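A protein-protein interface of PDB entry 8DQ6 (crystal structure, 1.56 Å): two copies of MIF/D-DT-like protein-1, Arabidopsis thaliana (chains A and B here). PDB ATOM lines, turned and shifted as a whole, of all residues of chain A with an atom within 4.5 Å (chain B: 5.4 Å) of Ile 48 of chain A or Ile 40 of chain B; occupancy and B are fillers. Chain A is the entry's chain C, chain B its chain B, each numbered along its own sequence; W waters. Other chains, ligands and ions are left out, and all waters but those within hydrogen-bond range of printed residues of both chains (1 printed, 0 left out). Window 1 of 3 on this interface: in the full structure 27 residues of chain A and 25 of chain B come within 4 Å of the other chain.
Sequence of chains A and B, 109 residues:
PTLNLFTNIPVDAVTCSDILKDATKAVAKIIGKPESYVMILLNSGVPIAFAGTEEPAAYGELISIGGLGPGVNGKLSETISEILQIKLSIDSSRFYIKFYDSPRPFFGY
Water W1 lies within hydrogen-bond range of the side-chain hydroxyl of Thr 24 of chain B, the backbone carbonyl oxygen of Val 38 of chain B, the backbone carbonyl oxygen of Ala 49 of chain A and the backbone NH of Phe 50 of chain A.
Printed residues of chain B within 4 Å of Phe 6 of chain A: Leu 41. Of the printed residues of chain B, Pro 47 of chain A touches Leu 20, Leu 41 and Leu 42. Of the printed residues of chain A, Leu 20 of chain B touches Pro 47, Ile 48, Ala 49 and Glu 54. Ala 23 of chain B touches none of the printed residues of chain A. Of the printed residues of chain A, Met 39 of chain B touches Ile 48, Ala 49 and Phe 50. Of the printed residues of chain A, Leu 42 of chain B touches Val 46 and Pro 47.
N of Ala 49 of chain A is in hydrogen-bond range of O of Ile 40 of chain B (2.9 Å). The backbone NH (N) of Leu 42 of chain B sits at hydrogen-bond distance from the backbone carbonyl oxygen (O) of Pro 47 of chain A (3.1 Å).
No position is printed for both chains.
Among the printed residues, pairs that only touch across the chains: Phe 6 of chain A with Leu 41 of chain B (3.5 Å), Val 46 of chain A with Leu 42 of chain B (3.8 Å), Pro 47 of chain A with Leu 20 of chain B (3.8 Å), Pro 47 of chain A with Leu 41 of chain B (3.4 Å), Ile 48 of chain A with Leu 20 of chain B (3.8 Å), Ile 48 of chain A with Met 39 of chain B (3.7 Å), Ile 48 of chain A with Ile 40 of chain B (3.2 Å), Ile 48 of chain A with Leu 41 of chain B (3.7 Å), Ala 49 of chain A with Leu 20 of chain B (3.8 Å), Ala 49 of chain A with Thr 24 of chain B (3.9 Å), Ala 49 of chain A with Val 38 of chain B (3.8 Å), Ala 49 of chain A with Met 39 of chain B (3.2 Å), Phe 50 of chain A with Val 38 of chain B (3.4 Å), Phe 50 of chain A with Met 39 of chain B (3.5 Å) and Glu 54 of chain A with Leu 20 of chain B (3.6 Å).
Of the 11 printed residues of chain A, 7 touch a printed residue of chain B. Of the 12 printed residues of chain B, 7 touch a printed residue of chain A. Hydrophobic or aromatic side chains of chain B that line the printed part of chain A: Leu 20, Met 39 and Leu 41. Along chain B the printed residues that touch a printed residue of chain A span positions 20 to 42.
The backbone carbonyl oxygen (O) of Leu 3 of chain B lies within hydrogen-bond range of the backbone NH (N) of Leu 41 of chain B (2.9 Å). The backbone NH of Leu 5 of chain B sits at hydrogen-bond distance from the backbone carbonyl oxygen of Leu 41 of chain B. The backbone carbonyl oxygen (O) of Leu 20 of chain B lies within hydrogen-bond range of the side-chain hydroxyl (OG1) of Thr 24 of chain B (2.8 Å). O of Glu 54 of chain A is in hydrogen-bond range of ND2 of Asn 8 of chain A, 3.4 Å away. The backbone NH of Leu 3 of chain B lies within hydrogen-bond range of the backbone carbonyl oxygen of Met 39 of chain B. O of Val 46 of chain A sits close to N of Asn 8 of chain A (3.4 Å).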
ATOM      1  N   PHE A   6     -17.005 -26.509  34.977  1.00  0.00           N
ATOM      2  CA  PHE A   6     -16.418 -26.548  33.635  1.00  0.00           C
ATOM      3  C   PHE A   6     -14.971 -26.095  33.731  1.00  0.00           C
ATOM      4  O   PHE A   6     -14.682 -25.115  34.418  1.00  0.00           O
ATOM      5  CB  PHE A   6     -17.151 -25.608  32.663  1.00  0.00           C
ATOM      6  CG  PHE A   6     -18.616 -25.921  32.470  1.00  0.00           C
ATOM      7  CD1 PHE A   6     -19.052 -26.541  31.301  1.00  0.00           C
ATOM      8  CD2 PHE A   6     -19.559 -25.570  33.439  1.00  0.00           C
ATOM      9  CE1 PHE A   6     -20.396 -26.830  31.106  1.00  0.00           C
ATOM     10  CE2 PHE A   6     -20.920 -25.852  33.260  1.00  0.00           C
ATOM     11  CZ  PHE A   6     -21.345 -26.487  32.081  1.00  0.00           C
ATOM     12  N   THR A   7     -14.056 -26.802  33.058  1.00  0.00           N
ATOM     13  CA  THR A   7     -12.659 -26.363  33.018  1.00  0.00           C
ATOM     14  C   THR A   7     -12.041 -26.673  31.659  1.00  0.00           C
ATOM     15  O   THR A   7     -12.406 -27.648  31.001  1.00  0.00           O
ATOM     16  CB  THR A   7     -11.801 -26.993  34.144  1.00  0.00           C
ATOM     17  OG1 THR A   7     -10.469 -26.456  34.089  1.00  0.00           O
ATOM     18  CG2 THR A   7     -11.730 -28.516  34.055  1.00  0.00           C
ATOM     19  N   ASN A   8     -11.082 -25.841  31.246  1.00  0.00           N
ATOM     20  CA  ASN A   8     -10.350 -26.131  30.013  1.00  0.00           C
ATOM     21  C   ASN A   8      -9.164 -27.060  30.219  1.00  0.00           C
ATOM     22  O   ASN A   8      -8.529 -27.439  29.231  1.00  0.00           O
ATOM     23  CB  ASN A   8      -9.886 -24.840  29.318  1.00  0.00           C
ATOM     24  CG  ASN A   8      -9.066 -23.927  30.214  1.00  0.00           C
ATOM     25  OD1 ASN A   8      -8.832 -24.212  31.384  1.00  0.00           O
ATOM     26  ND2 ASN A   8      -8.620 -22.804  29.648  1.00  0.00           N
ATOM     27  N   VAL A  46     -12.990 -28.452  28.232  1.00  0.00           N
ATOM     28  CA  VAL A  46     -13.902 -27.512  27.582  1.00  0.00           C
ATOM     29  C   VAL A  46     -13.123 -26.222  27.348  1.00  0.00           C
ATOM     30  O   VAL A  46     -12.769 -25.549  28.325  1.00  0.00           O
ATOM     31  CB  VAL A  46     -15.132 -27.242  28.463  1.00  0.00           C
ATOM     32  CG1 VAL A  46     -15.958 -26.115  27.874  1.00  0.00           C
ATOM     33  CG2 VAL A  46     -15.960 -28.493  28.642  1.00  0.00           C
ATOM     34  N   PRO A  47     -12.830 -25.841  26.106  1.00  0.00           N
ATOM     35  CA  PRO A  47     -12.061 -24.607  25.900  1.00  0.00           C
ATOM     36  C   PRO A  47     -12.759 -23.402  26.515  1.00  0.00           C
ATOM     37  O   PRO A  47     -13.979 -23.235  26.400  1.00  0.00           O
ATOM     38  CB  PRO A  47     -11.969 -24.497  24.377  1.00  0.00           C
ATOM     39  CG  PRO A  47     -12.089 -25.947  23.919  1.00  0.00           C
ATOM     40  CD  PRO A  47     -13.126 -26.526  24.838  1.00  0.00           C
ATOM     41  N   ILE A  48     -11.965 -22.581  27.195  1.00  0.00           N
ATOM     42  CA  ILE A  48     -12.443 -21.391  27.895  1.00  0.00           C
ATOM     43  C   ILE A  48     -11.495 -20.246  27.599  1.00  0.00           C
ATOM     44  O   ILE A  48     -10.275 -20.405  27.699  1.00  0.00           O
ATOM     45  CB  ILE A  48     -12.525 -21.587  29.419  1.00  0.00           C
ATOM     46  CG1 ILE A  48     -13.480 -22.739  29.764  1.00  0.00           C
ATOM     47  CG2 ILE A  48     -12.975 -20.271  30.092  1.00  0.00           C
ATOM     48  CD1 ILE A  48     -13.550 -23.060  31.250  1.00  0.00           C
ATOM     49  N   ALA A  49     -12.053 -19.093  27.257  1.00  0.00           N
ATOM     50  CA  ALA A  49     -11.316 -17.838  27.240  1.00  0.00           C
ATOM     51  C   ALA A  49     -11.804 -16.988  28.402  1.00  0.00           C
ATOM     52  O   ALA A  49     -13.012 -16.806  28.581  1.00  0.00           O
ATOM     53  CB  ALA A  49     -11.503 -17.081  25.920  1.00  0.00           C
ATOM     54  N   PHE A  50     -10.865 -16.484  29.195  1.00  0.00           N
ATOM     55  CA  PHE A  50     -11.195 -15.659  30.349  1.00  0.00           C
ATOM     56  C   PHE A  50     -10.205 -14.511  30.369  1.00  0.00           C
ATOM     57  O   PHE A  50      -8.993 -14.740  30.296  1.00  0.00           O
ATOM     58  CB  PHE A  50     -11.126 -16.465  31.659  1.00  0.00           C
ATOM     59  CG  PHE A  50     -11.780 -15.788  32.847  1.00  0.00           C
ATOM     60  CD1 PHE A  50     -12.647 -14.721  32.682  1.00  0.00           C
ATOM     61  CD2 PHE A  50     -11.530 -16.243  34.134  1.00  0.00           C
ATOM     62  CE1 PHE A  50     -13.247 -14.113  33.775  1.00  0.00           C
ATOM     63  CE2 PHE A  50     -12.128 -15.639  35.241  1.00  0.00           C
ATOM     64  CZ  PHE A  50     -12.986 -14.577  35.059  1.00  0.00           C
ATOM     65  N   THR A  53      -7.480 -14.535  27.522  1.00  0.00           N
ATOM     66  CA  THR A  53      -6.502 -15.598  27.311  1.00  0.00           C
ATOM     67  C   THR A  53      -7.166 -16.943  27.556  1.00  0.00           C
ATOM     68  O   THR A  53      -8.256 -17.033  28.126  1.00  0.00           O
ATOM     69  CB  THR A  53      -5.277 -15.489  28.229  1.00  0.00           C
ATOM     70  OG1 THR A  53      -5.632 -15.929  29.546  1.00  0.00           O
ATOM     71  CG2 THR A  53      -4.748 -14.056  28.296  1.00  0.00           C
ATOM     72  N   GLU A  54      -6.476 -17.998  27.138  1.00  0.00           N
ATOM     73  CA  GLU A  54      -6.922 -19.365  27.360  1.00  0.00           C
ATOM     74  C   GLU A  54      -6.071 -20.061  28.415  1.00  0.00           C
ATOM     75  O   GLU A  54      -5.851 -21.273  28.351  1.00  0.00           O
ATOM     76  CB  GLU A  54      -6.922 -20.152  26.051  1.00  0.00           C
ATOM     77  CG  GLU A  54      -8.060 -19.754  25.114  1.00  0.00           C
ATOM     78  CD  GLU A  54      -8.165 -20.679  23.920  1.00  0.00           C
ATOM     79  OE1 GLU A  54      -8.441 -21.878  24.118  1.00  0.00           O
ATOM     80  OE2 GLU A  54      -7.953 -20.209  22.783  1.00  0.00           O
ATOM     81  N   ALA A  57      -8.482 -22.304  33.554  1.00  0.00           N
ATOM     82  CA  ALA A  57      -9.622 -21.578  34.088  1.00  0.00           C
ATOM     83  C   ALA A  57     -10.714 -22.565  34.464  1.00  0.00           C
ATOM     84  O   ALA A  57     -10.786 -23.673  33.933  1.00  0.00           O
ATOM     85  CB  ALA A  57     -10.158 -20.559  33.080  1.00  0.00           C
ATOM     86  N   LEU B   3     -20.480 -16.320  28.619  1.00  0.00           N
ATOM     87  CA  LEU B   3     -21.210 -16.928  27.508  1.00  0.00           C
ATOM     88  C   LEU B   3     -20.827 -18.397  27.463  1.00  0.00           C
ATOM     89  O   LEU B   3     -19.683 -18.738  27.139  1.00  0.00           O
ATOM     90  CB  LEU B   3     -20.888 -16.239  26.187  1.00  0.00           C
ATOM     91  CG  LEU B   3     -21.528 -16.861  24.942  1.00  0.00           C
ATOM     92  CD1 LEU B   3     -23.037 -16.882  25.013  1.00  0.00           C
ATOM     93  CD2 LEU B   3     -21.081 -16.123  23.656  1.00  0.00           C
ATOM     94  N   LEU B   5     -21.429 -21.774  25.605  1.00  0.00           N
ATOM     95  CA  LEU B   5     -21.921 -22.254  24.324  1.00  0.00           C
ATOM     96  C   LEU B   5     -21.872 -23.771  24.279  1.00  0.00           C
ATOM     97  O   LEU B   5     -20.929 -24.390  24.785  1.00  0.00           O
ATOM     98  CB  LEU B   5     -21.078 -21.721  23.157  1.00  0.00           C
ATOM     99  CG  LEU B   5     -21.164 -20.222  22.903  1.00  0.00           C
ATOM    100  CD1 LEU B   5     -20.061 -19.803  21.914  1.00  0.00           C
ATOM    101  CD2 LEU B   5     -22.542 -19.826  22.383  1.00  0.00           C
ATOM    102  N   ILE B  19     -13.138 -18.692  17.710  1.00  0.00           N
ATOM    103  CA  ILE B  19     -14.475 -18.380  18.207  1.00  0.00           C
ATOM    104  C   ILE B  19     -14.384 -17.730  19.578  1.00  0.00           C
ATOM    105  O   ILE B  19     -15.058 -16.733  19.858  1.00  0.00           O
ATOM    106  CB  ILE B  19     -15.350 -19.650  18.241  1.00  0.00           C
ATOM    107  CG1 ILE B  19     -15.689 -20.115  16.820  1.00  0.00           C
ATOM    108  CG2 ILE B  19     -16.627 -19.388  19.018  1.00  0.00           C
ATOM    109  CD1 ILE B  19     -16.239 -21.518  16.773  1.00  0.00           C
ATOM    110  N   LEU B  20     -13.547 -18.289  20.449  1.00  0.00           N
ATOM    111  CA  LEU B  20     -13.398 -17.736  21.791  1.00  0.00           C
ATOM    112  C   LEU B  20     -12.898 -16.299  21.739  1.00  0.00           C
ATOM    113  O   LEU B  20     -13.382 -15.438  22.484  1.00  0.00           O
ATOM    114  CB  LEU B  20     -12.440 -18.596  22.607  1.00  0.00           C
ATOM    115  CG  LEU B  20     -12.887 -20.020  22.913  1.00  0.00           C
ATOM    116  CD1 LEU B  20     -11.873 -20.696  23.832  1.00  0.00           C
ATOM    117  CD2 LEU B  20     -14.269 -20.017  23.520  1.00  0.00           C
ATOM    118  N   ALA B  23     -15.655 -13.967  20.093  1.00  0.00           N
ATOM    119  CA  ALA B  23     -16.761 -13.800  21.030  1.00  0.00           C
ATOM    120  C   ALA B  23     -16.368 -12.898  22.197  1.00  0.00           C
ATOM    121  O   ALA B  23     -17.177 -12.083  22.655  1.00  0.00           O
ATOM    122  CB  ALA B  23     -17.233 -15.169  21.539  1.00  0.00           C
ATOM    123  N   THR B  24     -15.129 -13.022  22.678  1.00  0.00           N
ATOM    124  CA  THR B  24     -14.649 -12.126  23.732  1.00  0.00           C
ATOM    125  C   THR B  24     -14.706 -10.670  23.282  1.00  0.00           C
ATOM    126  O   THR B  24     -15.231  -9.811  23.998  1.00  0.00           O
ATOM    127  CB  THR B  24     -13.228 -12.507  24.141  1.00  0.00           C
ATOM    128  OG1 THR B  24     -13.232 -13.815  24.726  1.00  0.00           O
ATOM    129  CG2 THR B  24     -12.666 -11.504  25.168  1.00  0.00           C
ATOM    130  N   VAL B  27     -18.568  -9.540  22.829  1.00  0.00           N
ATOM    131  CA  VAL B  27     -19.280  -9.365  24.091  1.00  0.00           C
ATOM    132  C   VAL B  27     -18.750  -8.144  24.836  1.00  0.00           C
ATOM    133  O   VAL B  27     -19.526  -7.340  25.366  1.00  0.00           O
ATOM    134  CB  VAL B  27     -19.183 -10.644  24.948  1.00  0.00           C
ATOM    135  CG1 VAL B  27     -19.760 -10.405  26.337  1.00  0.00           C
ATOM    136  CG2 VAL B  27     -19.922 -11.793  24.273  1.00  0.00           C
ATOM    137  N   VAL B  38     -14.942 -10.887  30.833  1.00  0.00           N
ATOM    138  CA  VAL B  38     -15.635 -11.729  29.859  1.00  0.00           C
ATOM    139  C   VAL B  38     -15.065 -13.136  29.899  1.00  0.00           C
ATOM    140  O   VAL B  38     -13.850 -13.329  29.794  1.00  0.00           O
ATOM    141  CB  VAL B  38     -15.530 -11.141  28.441  1.00  0.00           C
ATOM    142  CG1 VAL B  38     -16.094 -12.103  27.410  1.00  0.00           C
ATOM    143  CG2 VAL B  38     -16.260  -9.801  28.384  1.00  0.00           C
ATOM    144  N   MET B  39     -15.949 -14.123  30.041  1.00  0.00           N
ATOM    145  CA  MET B  39     -15.588 -15.531  29.939  1.00  0.00           C
ATOM    146  C   MET B  39     -16.455 -16.159  28.861  1.00  0.00           C
ATOM    147  O   MET B  39     -17.666 -15.929  28.837  1.00  0.00           O
ATOM    148  CB  MET B  39     -15.767 -16.254  31.283  1.00  0.00           C
ATOM    149  CG  MET B  39     -15.476 -17.751  31.217  1.00  0.00           C
ATOM    150  SD  MET B  39     -15.876 -18.594  32.767  1.00  0.00           S
ATOM    151  CE  MET B  39     -14.329 -18.357  33.617  1.00  0.00           C
ATOM    152  N   ILE B  40     -15.820 -16.888  27.937  1.00  0.00           N
ATOM    153  CA  ILE B  40     -16.503 -17.662  26.905  1.00  0.00           C
ATOM    154  C   ILE B  40     -16.098 -19.124  27.062  1.00  0.00           C
ATOM    155  O   ILE B  40     -14.909 -19.429  27.213  1.00  0.00           O
ATOM    156  CB  ILE B  40     -16.143 -17.185  25.483  1.00  0.00           C
ATOM    157  CG1 ILE B  40     -16.070 -15.659  25.401  1.00  0.00           C
ATOM    158  CG2 ILE B  40     -17.137 -17.742  24.467  1.00  0.00           C
ATOM    159  CD1 ILE B  40     -17.422 -14.988  25.489  1.00  0.00           C
ATOM    160  N   LEU B  41     -17.080 -20.025  26.991  1.00  0.00           N
ATOM    161  CA  LEU B  41     -16.839 -21.465  26.976  1.00  0.00           C
ATOM    162  C   LEU B  41     -17.437 -22.041  25.710  1.00  0.00           C
ATOM    163  O   LEU B  41     -18.507 -21.615  25.272  1.00  0.00           O
ATOM    164  CB  LEU B  41     -17.479 -22.171  28.181  1.00  0.00           C
ATOM    165  CG  LEU B  41     -17.144 -21.655  29.582  1.00  0.00           C
ATOM    166  CD1 LEU B  41     -18.148 -20.607  30.031  1.00  0.00           C
ATOM    167  CD2 LEU B  41     -17.132 -22.814  30.563  1.00  0.00           C
ATOM    168  N   LEU B  42     -16.774 -23.048  25.141  1.00  0.00           N
ATOM    169  CA  LEU B  42     -17.329 -23.734  23.975  1.00  0.00           C
ATOM    170  C   LEU B  42     -17.335 -25.235  24.241  1.00  0.00           C
ATOM    171  O   LEU B  42     -16.298 -25.900  24.133  1.00  0.00           O
ATOM    172  CB  LEU B  42     -16.541 -23.389  22.706  1.00  0.00           C
ATOM    173  CG  LEU B  42     -17.064 -23.967  21.384  1.00  0.00           C
ATOM    174  CD1 LEU B  42     -18.535 -23.728  21.172  1.00  0.00           C
ATOM    175  CD2 LEU B  42     -16.280 -23.384  20.194  1.00  0.00           C
HETATM  176  O   HOH W   1     -12.193 -13.830  27.441  1.00  0.00           O
